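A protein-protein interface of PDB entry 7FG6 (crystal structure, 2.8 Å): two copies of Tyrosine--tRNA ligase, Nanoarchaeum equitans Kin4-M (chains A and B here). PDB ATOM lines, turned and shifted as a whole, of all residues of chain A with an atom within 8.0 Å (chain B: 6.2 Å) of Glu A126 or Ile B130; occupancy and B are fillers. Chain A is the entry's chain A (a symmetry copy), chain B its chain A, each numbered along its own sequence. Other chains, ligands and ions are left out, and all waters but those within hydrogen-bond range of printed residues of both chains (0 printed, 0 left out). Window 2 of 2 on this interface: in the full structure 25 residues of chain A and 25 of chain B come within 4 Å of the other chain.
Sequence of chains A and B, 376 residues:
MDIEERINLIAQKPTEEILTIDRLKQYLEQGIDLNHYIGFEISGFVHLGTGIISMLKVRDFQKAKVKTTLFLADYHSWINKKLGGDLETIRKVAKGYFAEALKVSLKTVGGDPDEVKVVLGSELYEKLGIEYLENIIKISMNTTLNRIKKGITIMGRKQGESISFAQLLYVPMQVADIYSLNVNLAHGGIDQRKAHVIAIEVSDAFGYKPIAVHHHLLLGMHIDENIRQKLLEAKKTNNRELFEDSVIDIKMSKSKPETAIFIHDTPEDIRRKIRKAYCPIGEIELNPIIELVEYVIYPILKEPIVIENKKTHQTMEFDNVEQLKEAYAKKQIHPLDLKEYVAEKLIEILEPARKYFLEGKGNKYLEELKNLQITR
Printed residues of chain B within 4 Å of Glu A126: Ile B130. Of chain A, only Tyr A75, Tyr A125 and Glu A126 come within 4 Å of Ile B130. Gly B129 touches none of the printed residues of chain A. Printed residues of chain B within 4 Å of Tyr A132: Leu B133. Of the printed residues of chain B, Tyr A125 touches Ile B130 (3.5 Å) and Leu B133 (3.97 Å). Of the printed residues of chain B, Tyr A75 touches Ile B130, Leu B133 and Glu B134. Leu B128 touches none of the printed residues of chain A. The nearest residue of chain A that does not touch Ile B130 is Ser A122 (4.1 Å). The nearest printed residue of chain A that does not touch Leu B133 is Trp A78 (5.6 Å).
Tyr A75 touches Ile B130 (OH to CG2, 3.1 Å). Tyr A75 touches Leu B133. C of Tyr A125 touches CD1 of Ile B130, 3.5 Å away. Leu B133 touches Tyr A125 (CD2 to CD2, 3.97 Å). Glu A126 touches Ile B130 (N to CD1, 3.4 Å). CD1 of Ile A130 touches C of Tyr B125, at 3.5 Å. CD2 of Leu B133 touches CE2 of Tyr A132 (3.8 Å).
The side-chain hydroxyl (OH) of Tyr B132 sits close to the side-chain hydroxyl (OH) of Tyr B125 (3.3 Å). OH of Tyr A125 lies close to OH of Tyr A132 (3.3 Å).
Tyr A125 touches Ile B130, and with the chains exchanged Ile A130 touches Tyr B125. Positions printed for both chains: 125, 128, 129, 130 and 132. Of the 8 pairs that touch across the chains among the printed residues, 2 have their exchanged pair printed and touching as well.
The side-chain carboxylate (OE2) of Glu B134 is in hydrogen-bond range of the side-chain hydroxyl (OH) of Tyr A75 (2.8 Å).
Of the 9 printed residues of chain B, 4 touch a printed residue of chain A.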
ATOM      1  N   TYR A  75      25.227  12.914  -4.690  1.00  0.00           N
ATOM      2  CA  TYR A  75      25.084  12.391  -6.045  1.00  0.00           C
ATOM      3  C   TYR A  75      25.601  13.387  -7.069  1.00  0.00           C
ATOM      4  O   TYR A  75      26.176  13.000  -8.095  1.00  0.00           O
ATOM      5  CB  TYR A  75      23.623  12.057  -6.328  1.00  0.00           C
ATOM      6  CG  TYR A  75      23.232  10.689  -5.848  1.00  0.00           C
ATOM      7  CD1 TYR A  75      21.956  10.193  -6.065  1.00  0.00           C
ATOM      8  CD2 TYR A  75      24.143   9.892  -5.173  1.00  0.00           C
ATOM      9  CE1 TYR A  75      21.600   8.940  -5.621  1.00  0.00           C
ATOM     10  CE2 TYR A  75      23.799   8.643  -4.727  1.00  0.00           C
ATOM     11  CZ  TYR A  75      22.529   8.170  -4.953  1.00  0.00           C
ATOM     12  OH  TYR A  75      22.190   6.920  -4.502  1.00  0.00           O
ATOM     13  N   TRP A  78      29.212  13.011  -7.026  1.00  0.00           N
ATOM     14  CA  TRP A  78      29.574  11.730  -7.621  1.00  0.00           C
ATOM     15  C   TRP A  78      29.479  11.770  -9.140  1.00  0.00           C
ATOM     16  O   TRP A  78      30.199  11.035  -9.825  1.00  0.00           O
ATOM     17  CB  TRP A  78      28.682  10.628  -7.048  1.00  0.00           C
ATOM     18  CG  TRP A  78      28.889   9.284  -7.666  1.00  0.00           C
ATOM     19  CD1 TRP A  78      30.076   8.637  -7.848  1.00  0.00           C
ATOM     20  CD2 TRP A  78      27.875   8.411  -8.171  1.00  0.00           C
ATOM     21  NE1 TRP A  78      29.865   7.417  -8.443  1.00  0.00           N
ATOM     22  CE2 TRP A  78      28.520   7.255  -8.651  1.00  0.00           C
ATOM     23  CE3 TRP A  78      26.482   8.496  -8.268  1.00  0.00           C
ATOM     24  CZ2 TRP A  78      27.821   6.194  -9.217  1.00  0.00           C
ATOM     25  CZ3 TRP A  78      25.793   7.443  -8.829  1.00  0.00           C
ATOM     26  CH2 TRP A  78      26.461   6.308  -9.295  1.00  0.00           C
ATOM     27  N   LEU A  87      31.570   7.034  -4.105  1.00  0.00           N
ATOM     28  CA  LEU A  87      30.378   7.549  -3.436  1.00  0.00           C
ATOM     29  C   LEU A  87      30.524   7.505  -1.921  1.00  0.00           C
ATOM     30  O   LEU A  87      30.139   8.454  -1.228  1.00  0.00           O
ATOM     31  CB  LEU A  87      29.147   6.758  -3.883  1.00  0.00           C
ATOM     32  CG  LEU A  87      27.784   7.299  -3.448  1.00  0.00           C
ATOM     33  CD1 LEU A  87      27.660   8.779  -3.774  1.00  0.00           C
ATOM     34  CD2 LEU A  87      26.664   6.508  -4.103  1.00  0.00           C
ATOM     35  N   ARG A  91      30.462  10.582   0.932  1.00  0.00           N
ATOM     36  CA  ARG A  91      29.378  10.561   1.915  1.00  0.00           C
ATOM     37  C   ARG A  91      29.861  10.854   3.326  1.00  0.00           C
ATOM     38  O   ARG A  91      29.091  11.355   4.151  1.00  0.00           O
ATOM     39  CB  ARG A  91      28.657   9.210   1.879  1.00  0.00           C
ATOM     40  CG  ARG A  91      27.730   9.045   0.685  1.00  0.00           C
ATOM     41  CD  ARG A  91      27.097   7.666   0.659  1.00  0.00           C
ATOM     42  NE  ARG A  91      25.779   7.664   0.027  1.00  0.00           N
ATOM     43  CZ  ARG A  91      25.314   6.667  -0.717  1.00  0.00           C
ATOM     44  NH1 ARG A  91      26.061   5.590  -0.923  1.00  0.00           N
ATOM     45  NH2 ARG A  91      24.105   6.740  -1.258  1.00  0.00           N
ATOM     46  N   LEU A 120      21.217  15.149   3.694  1.00  0.00           N
ATOM     47  CA  LEU A 120      22.019  14.473   2.687  1.00  0.00           C
ATOM     48  C   LEU A 120      21.158  14.119   1.480  1.00  0.00           C
ATOM     49  O   LEU A 120      19.959  13.851   1.602  1.00  0.00           O
ATOM     50  CB  LEU A 120      22.658  13.210   3.268  1.00  0.00           C
ATOM     51  CG  LEU A 120      23.676  12.478   2.390  1.00  0.00           C
ATOM     52  CD1 LEU A 120      24.836  13.395   2.031  1.00  0.00           C
ATOM     53  CD2 LEU A 120      24.179  11.218   3.080  1.00  0.00           C
ATOM     54  N   GLY A 121      21.785  14.127   0.302  1.00  0.00           N
ATOM     55  CA  GLY A 121      21.040  13.867  -0.920  1.00  0.00           C
ATOM     56  C   GLY A 121      20.487  12.456  -0.983  1.00  0.00           C
ATOM     57  O   GLY A 121      19.324  12.248  -1.339  1.00  0.00           O
ATOM     58  N   SER A 122      21.312  11.466  -0.630  1.00  0.00           N
ATOM     59  CA  SER A 122      20.884  10.074  -0.729  1.00  0.00           C
ATOM     60  C   SER A 122      19.741   9.772   0.232  1.00  0.00           C
ATOM     61  O   SER A 122      18.776   9.089  -0.135  1.00  0.00           O
ATOM     62  CB  SER A 122      22.065   9.143  -0.465  1.00  0.00           C
ATOM     63  OG  SER A 122      23.125   9.396  -1.371  1.00  0.00           O
ATOM     64  N   GLU A 123      19.832  10.267   1.468  1.00  0.00           N
ATOM     65  CA  GLU A 123      18.775  10.016   2.442  1.00  0.00           C
ATOM     66  C   GLU A 123      17.469  10.678   2.024  1.00  0.00           C
ATOM     67  O   GLU A 123      16.385  10.137   2.272  1.00  0.00           O
ATOM     68  CB  GLU A 123      19.205  10.505   3.823  1.00  0.00           C
ATOM     69  CG  GLU A 123      20.514   9.910   4.311  1.00  0.00           C
ATOM     70  CD  GLU A 123      21.071  10.641   5.516  1.00  0.00           C
ATOM     71  OE1 GLU A 123      20.561  11.735   5.835  1.00  0.00           O
ATOM     72  OE2 GLU A 123      22.017  10.120   6.143  1.00  0.00           O
ATOM     73  N   LEU A 124      17.550  11.847   1.387  1.00  0.00           N
ATOM     74  CA  LEU A 124      16.343  12.523   0.924  1.00  0.00           C
ATOM     75  C   LEU A 124      15.691  11.756  -0.220  1.00  0.00           C
ATOM     76  O   LEU A 124      14.469  11.564  -0.236  1.00  0.00           O
ATOM     77  CB  LEU A 124      16.670  13.952   0.495  1.00  0.00           C
ATOM     78  CG  LEU A 124      15.558  14.662  -0.278  1.00  0.00           C
ATOM     79  CD1 LEU A 124      14.361  14.902   0.628  1.00  0.00           C
ATOM     80  CD2 LEU A 124      16.054  15.965  -0.881  1.00  0.00           C
ATOM     81  N   TYR A 125      16.493  11.310  -1.190  1.00  0.00           N
ATOM     82  CA  TYR A 125      15.938  10.575  -2.321  1.00  0.00           C
ATOM     83  C   TYR A 125      15.384   9.224  -1.890  1.00  0.00           C
ATOM     84  O   TYR A 125      14.414   8.737  -2.480  1.00  0.00           O
ATOM     85  CB  TYR A 125      16.999  10.389  -3.410  1.00  0.00           C
ATOM     86  CG  TYR A 125      17.716  11.654  -3.839  1.00  0.00           C
ATOM     87  CD1 TYR A 125      17.116  12.902  -3.710  1.00  0.00           C
ATOM     88  CD2 TYR A 125      18.994  11.596  -4.380  1.00  0.00           C
ATOM     89  CE1 TYR A 125      17.774  14.054  -4.099  1.00  0.00           C
ATOM     90  CE2 TYR A 125      19.656  12.742  -4.774  1.00  0.00           C
ATOM     91  CZ  TYR A 125      19.042  13.968  -4.634  1.00  0.00           C
ATOM     92  OH  TYR A 125      19.699  15.111  -5.025  1.00  0.00           O
ATOM     93  N   GLU A 126      15.980   8.607  -0.866  1.00  0.00           N
ATOM     94  CA  GLU A 126      15.459   7.341  -0.359  1.00  0.00           C
ATOM     95  C   GLU A 126      14.159   7.550   0.407  1.00  0.00           C
ATOM     96  O   GLU A 126      13.245   6.721   0.332  1.00  0.00           O
ATOM     97  CB  GLU A 126      16.501   6.662   0.530  1.00  0.00           C
ATOM     98  CG  GLU A 126      16.224   5.191   0.787  1.00  0.00           C
ATOM     99  CD  GLU A 126      17.376   4.498   1.484  1.00  0.00           C
ATOM    100  OE1 GLU A 126      18.189   5.197   2.125  1.00  0.00           O
ATOM    101  OE2 GLU A 126      17.472   3.257   1.389  1.00  0.00           O
ATOM    102  N   LYS A 127      14.067   8.648   1.162  1.00  0.00           N
ATOM    103  CA  LYS A 127      12.842   8.974   1.888  1.00  0.00           C
ATOM    104  C   LYS A 127      11.678   9.201   0.937  1.00  0.00           C
ATOM    105  O   LYS A 127      10.589   8.644   1.124  1.00  0.00           O
ATOM    106  CB  LYS A 127      13.079  10.205   2.771  1.00  0.00           C
ATOM    107  CG  LYS A 127      11.920  10.638   3.658  1.00  0.00           C
ATOM    108  CD  LYS A 127      11.083  11.675   2.918  1.00  0.00           C
ATOM    109  CE  LYS A 127       9.967  12.253   3.771  1.00  0.00           C
ATOM    110  NZ  LYS A 127       9.196  13.226   2.952  1.00  0.00           N
ATOM    111  N   LEU A 128      11.881  10.036  -0.078  1.00  0.00           N
ATOM    112  CA  LEU A 128      10.795  10.319  -1.009  1.00  0.00           C
ATOM    113  C   LEU A 128      10.561   9.146  -1.950  1.00  0.00           C
ATOM    114  O   LEU A 128       9.411   8.794  -2.241  1.00  0.00           O
ATOM    115  CB  LEU A 128      11.089  11.594  -1.799  1.00  0.00           C
ATOM    116  CG  LEU A 128      11.378  12.861  -0.993  1.00  0.00           C
ATOM    117  CD1 LEU A 128      11.994  13.900  -1.904  1.00  0.00           C
ATOM    118  CD2 LEU A 128      10.104  13.388  -0.354  1.00  0.00           C
ATOM    119  N   GLY A 129      11.636   8.525  -2.424  1.00  0.00           N
ATOM    120  CA  GLY A 129      11.526   7.384  -3.305  1.00  0.00           C
ATOM    121  C   GLY A 129      11.034   7.736  -4.693  1.00  0.00           C
ATOM    122  O   GLY A 129      11.801   8.220  -5.530  1.00  0.00           O
ATOM    123  N   ILE A 130       9.746   7.499  -4.943  1.00  0.00           N
ATOM    124  CA  ILE A 130       9.194   7.679  -6.282  1.00  0.00           C
ATOM    125  C   ILE A 130       8.931   9.151  -6.574  1.00  0.00           C
ATOM    126  O   ILE A 130       9.111   9.610  -7.708  1.00  0.00           O
ATOM    127  CB  ILE A 130       7.924   6.825  -6.438  1.00  0.00           C
ATOM    128  CG1 ILE A 130       8.301   5.352  -6.568  1.00  0.00           C
ATOM    129  CG2 ILE A 130       7.108   7.266  -7.639  1.00  0.00           C
ATOM    130  CD1 ILE A 130       9.315   5.091  -7.652  1.00  0.00           C
ATOM    131  N   TYR A 132      10.600  11.700  -5.991  1.00  0.00           N
ATOM    132  CA  TYR A 132      11.774  12.362  -6.549  1.00  0.00           C
ATOM    133  C   TYR A 132      11.909  12.076  -8.040  1.00  0.00           C
ATOM    134  O   TYR A 132      12.144  12.991  -8.838  1.00  0.00           O
ATOM    135  CB  TYR A 132      13.033  11.924  -5.801  1.00  0.00           C
ATOM    136  CG  TYR A 132      14.287  12.615  -6.284  1.00  0.00           C
ATOM    137  CD1 TYR A 132      14.400  13.999  -6.241  1.00  0.00           C
ATOM    138  CD2 TYR A 132      15.356  11.886  -6.789  1.00  0.00           C
ATOM    139  CE1 TYR A 132      15.541  14.637  -6.685  1.00  0.00           C
ATOM    140  CE2 TYR A 132      16.503  12.516  -7.233  1.00  0.00           C
ATOM    141  CZ  TYR A 132      16.590  13.892  -7.182  1.00  0.00           C
ATOM    142  OH  TYR A 132      17.729  14.525  -7.621  1.00  0.00           O
ATOM    143  N   TYR B 125      10.243   0.504  -9.556  1.00  0.00           N
ATOM    144  CA  TYR B 125      11.079   1.619  -9.126  1.00  0.00           C
ATOM    145  C   TYR B 125      10.867   1.939  -7.652  1.00  0.00           C
ATOM    146  O   TYR B 125      11.802   2.379  -6.974  1.00  0.00           O
ATOM    147  CB  TYR B 125      10.802   2.858  -9.981  1.00  0.00           C
ATOM    148  CG  TYR B 125      10.861   2.636 -11.480  1.00  0.00           C
ATOM    149  CD1 TYR B 125      11.630   1.616 -12.029  1.00  0.00           C
ATOM    150  CD2 TYR B 125      10.149   3.456 -12.347  1.00  0.00           C
ATOM    151  CE1 TYR B 125      11.678   1.414 -13.396  1.00  0.00           C
ATOM    152  CE2 TYR B 125      10.196   3.264 -13.714  1.00  0.00           C
ATOM    153  CZ  TYR B 125      10.963   2.243 -14.234  1.00  0.00           C
ATOM    154  OH  TYR B 125      11.011   2.049 -15.594  1.00  0.00           O
ATOM    155  N   LEU B 128      12.831  -0.943  -5.640  1.00  0.00           N
ATOM    156  CA  LEU B 128      14.274  -0.745  -5.598  1.00  0.00           C
ATOM    157  C   LEU B 128      14.626   0.585  -4.949  1.00  0.00           C
ATOM    158  O   LEU B 128      15.574   0.668  -4.159  1.00  0.00           O
ATOM    159  CB  LEU B 128      14.865  -0.831  -7.005  1.00  0.00           C
ATOM    160  CG  LEU B 128      14.574  -2.100  -7.806  1.00  0.00           C
ATOM    161  CD1 LEU B 128      14.910  -1.859  -9.261  1.00  0.00           C
ATOM    162  CD2 LEU B 128      15.368  -3.272  -7.254  1.00  0.00           C
ATOM    163  N   GLY B 129      13.865   1.631  -5.259  1.00  0.00           N
ATOM    164  CA  GLY B 129      14.097   2.935  -4.678  1.00  0.00           C
ATOM    165  C   GLY B 129      15.354   3.610  -5.188  1.00  0.00           C
ATOM    166  O   GLY B 129      15.365   4.174  -6.286  1.00  0.00           O
ATOM    167  N   ILE B 130      16.422   3.552  -4.392  1.00  0.00           N
ATOM    168  CA  ILE B 130      17.645   4.276  -4.723  1.00  0.00           C
ATOM    169  C   ILE B 130      18.452   3.534  -5.781  1.00  0.00           C
ATOM    170  O   ILE B 130      19.077   4.158  -6.647  1.00  0.00           O
ATOM    171  CB  ILE B 130      18.463   4.521  -3.443  1.00  0.00           C
ATOM    172  CG1 ILE B 130      17.801   5.610  -2.604  1.00  0.00           C
ATOM    173  CG2 ILE B 130      19.894   4.907  -3.770  1.00  0.00           C
ATOM    174  CD1 ILE B 130      17.534   6.877  -3.377  1.00  0.00           C
ATOM    175  N   GLU B 131      18.446   2.199  -5.736  1.00  0.00           N
ATOM    176  CA  GLU B 131      19.231   1.417  -6.686  1.00  0.00           C
ATOM    177  C   GLU B 131      18.860   1.738  -8.128  1.00  0.00           C
ATOM    178  O   GLU B 131      19.720   1.689  -9.016  1.00  0.00           O
ATOM    179  CB  GLU B 131      19.052  -0.076  -6.410  1.00  0.00           C
ATOM    180  CG  GLU B 131      19.900  -0.980  -7.290  1.00  0.00           C
ATOM    181  CD  GLU B 131      19.651  -2.452  -7.028  1.00  0.00           C
ATOM    182  OE1 GLU B 131      19.091  -2.781  -5.962  1.00  0.00           O
ATOM    183  OE2 GLU B 131      20.014  -3.280  -7.890  1.00  0.00           O
ATOM    184  N   TYR B 132      17.596   2.079  -8.383  1.00  0.00           N
ATOM    185  CA  TYR B 132      17.190   2.451  -9.735  1.00  0.00           C
ATOM    186  C   TYR B 132      17.825   3.771 -10.155  1.00  0.00           C
ATOM    187  O   TYR B 132      18.358   3.889 -11.264  1.00  0.00           O
ATOM    188  CB  TYR B 132      15.667   2.533  -9.825  1.00  0.00           C
ATOM    189  CG  TYR B 132      15.166   2.855 -11.214  1.00  0.00           C
ATOM    190  CD1 TYR B 132      15.470   2.031 -12.290  1.00  0.00           C
ATOM    191  CD2 TYR B 132      14.396   3.986 -11.452  1.00  0.00           C
ATOM    192  CE1 TYR B 132      15.018   2.322 -13.562  1.00  0.00           C
ATOM    193  CE2 TYR B 132      13.939   4.284 -12.722  1.00  0.00           C
ATOM    194  CZ  TYR B 132      14.256   3.450 -13.774  1.00  0.00           C
ATOM    195  OH  TYR B 132      13.804   3.740 -15.040  1.00  0.00           O
ATOM    196  N   LEU B 133      17.775   4.778  -9.279  1.00  0.00           N
ATOM    197  CA  LEU B 133      18.392   6.061  -9.598  1.00  0.00           C
ATOM    198  C   LEU B 133      19.905   5.942  -9.716  1.00  0.00           C
ATOM    199  O   LEU B 133      20.518   6.638 -10.534  1.00  0.00           O
ATOM    200  CB  LEU B 133      18.024   7.103  -8.541  1.00  0.00           C
ATOM    201  CG  LEU B 133      18.333   8.558  -8.902  1.00  0.00           C
ATOM    202  CD1 LEU B 133      17.185   9.171  -9.691  1.00  0.00           C
ATOM    203  CD2 LEU B 133      18.627   9.376  -7.653  1.00  0.00           C
ATOM    204  N   GLU B 134      20.522   5.071  -8.914  1.00  0.00           N
ATOM    205  CA  GLU B 134      21.959   4.846  -9.038  1.00  0.00           C
ATOM    206  C   GLU B 134      22.302   4.235 -10.389  1.00  0.00           C
ATOM    207  O   GLU B 134      23.260   4.660 -11.047  1.00  0.00           O
ATOM    208  CB  GLU B 134      22.451   3.946  -7.904  1.00  0.00           C
ATOM    209  CG  GLU B 134      22.405   4.603  -6.539  1.00  0.00           C
ATOM    210  CD  GLU B 134      23.151   3.814  -5.481  1.00  0.00           C
ATOM    211  OE1 GLU B 134      23.625   2.700  -5.789  1.00  0.00           O
ATOM    212  OE2 GLU B 134      23.262   4.311  -4.341  1.00  0.00           O
ATOM    213  N   ASN B 135      21.526   3.237 -10.821  1.00  0.00           N
ATOM    214  CA  ASN B 135      21.770   2.619 -12.121  1.00  0.00           C
ATOM    215  C   ASN B 135      21.618   3.632 -13.248  1.00  0.00           C
ATOM    216  O   ASN B 135      22.386   3.611 -14.216  1.00  0.00           O
ATOM    217  CB  ASN B 135      20.820   1.438 -12.325  1.00  0.00           C
ATOM    218  CG  ASN B 135      21.085   0.302 -11.356  1.00  0.00           C
ATOM    219  OD1 ASN B 135      22.177   0.189 -10.798  1.00  0.00           O
ATOM    220  ND2 ASN B 135      20.085  -0.547 -11.151  1.00  0.00           N
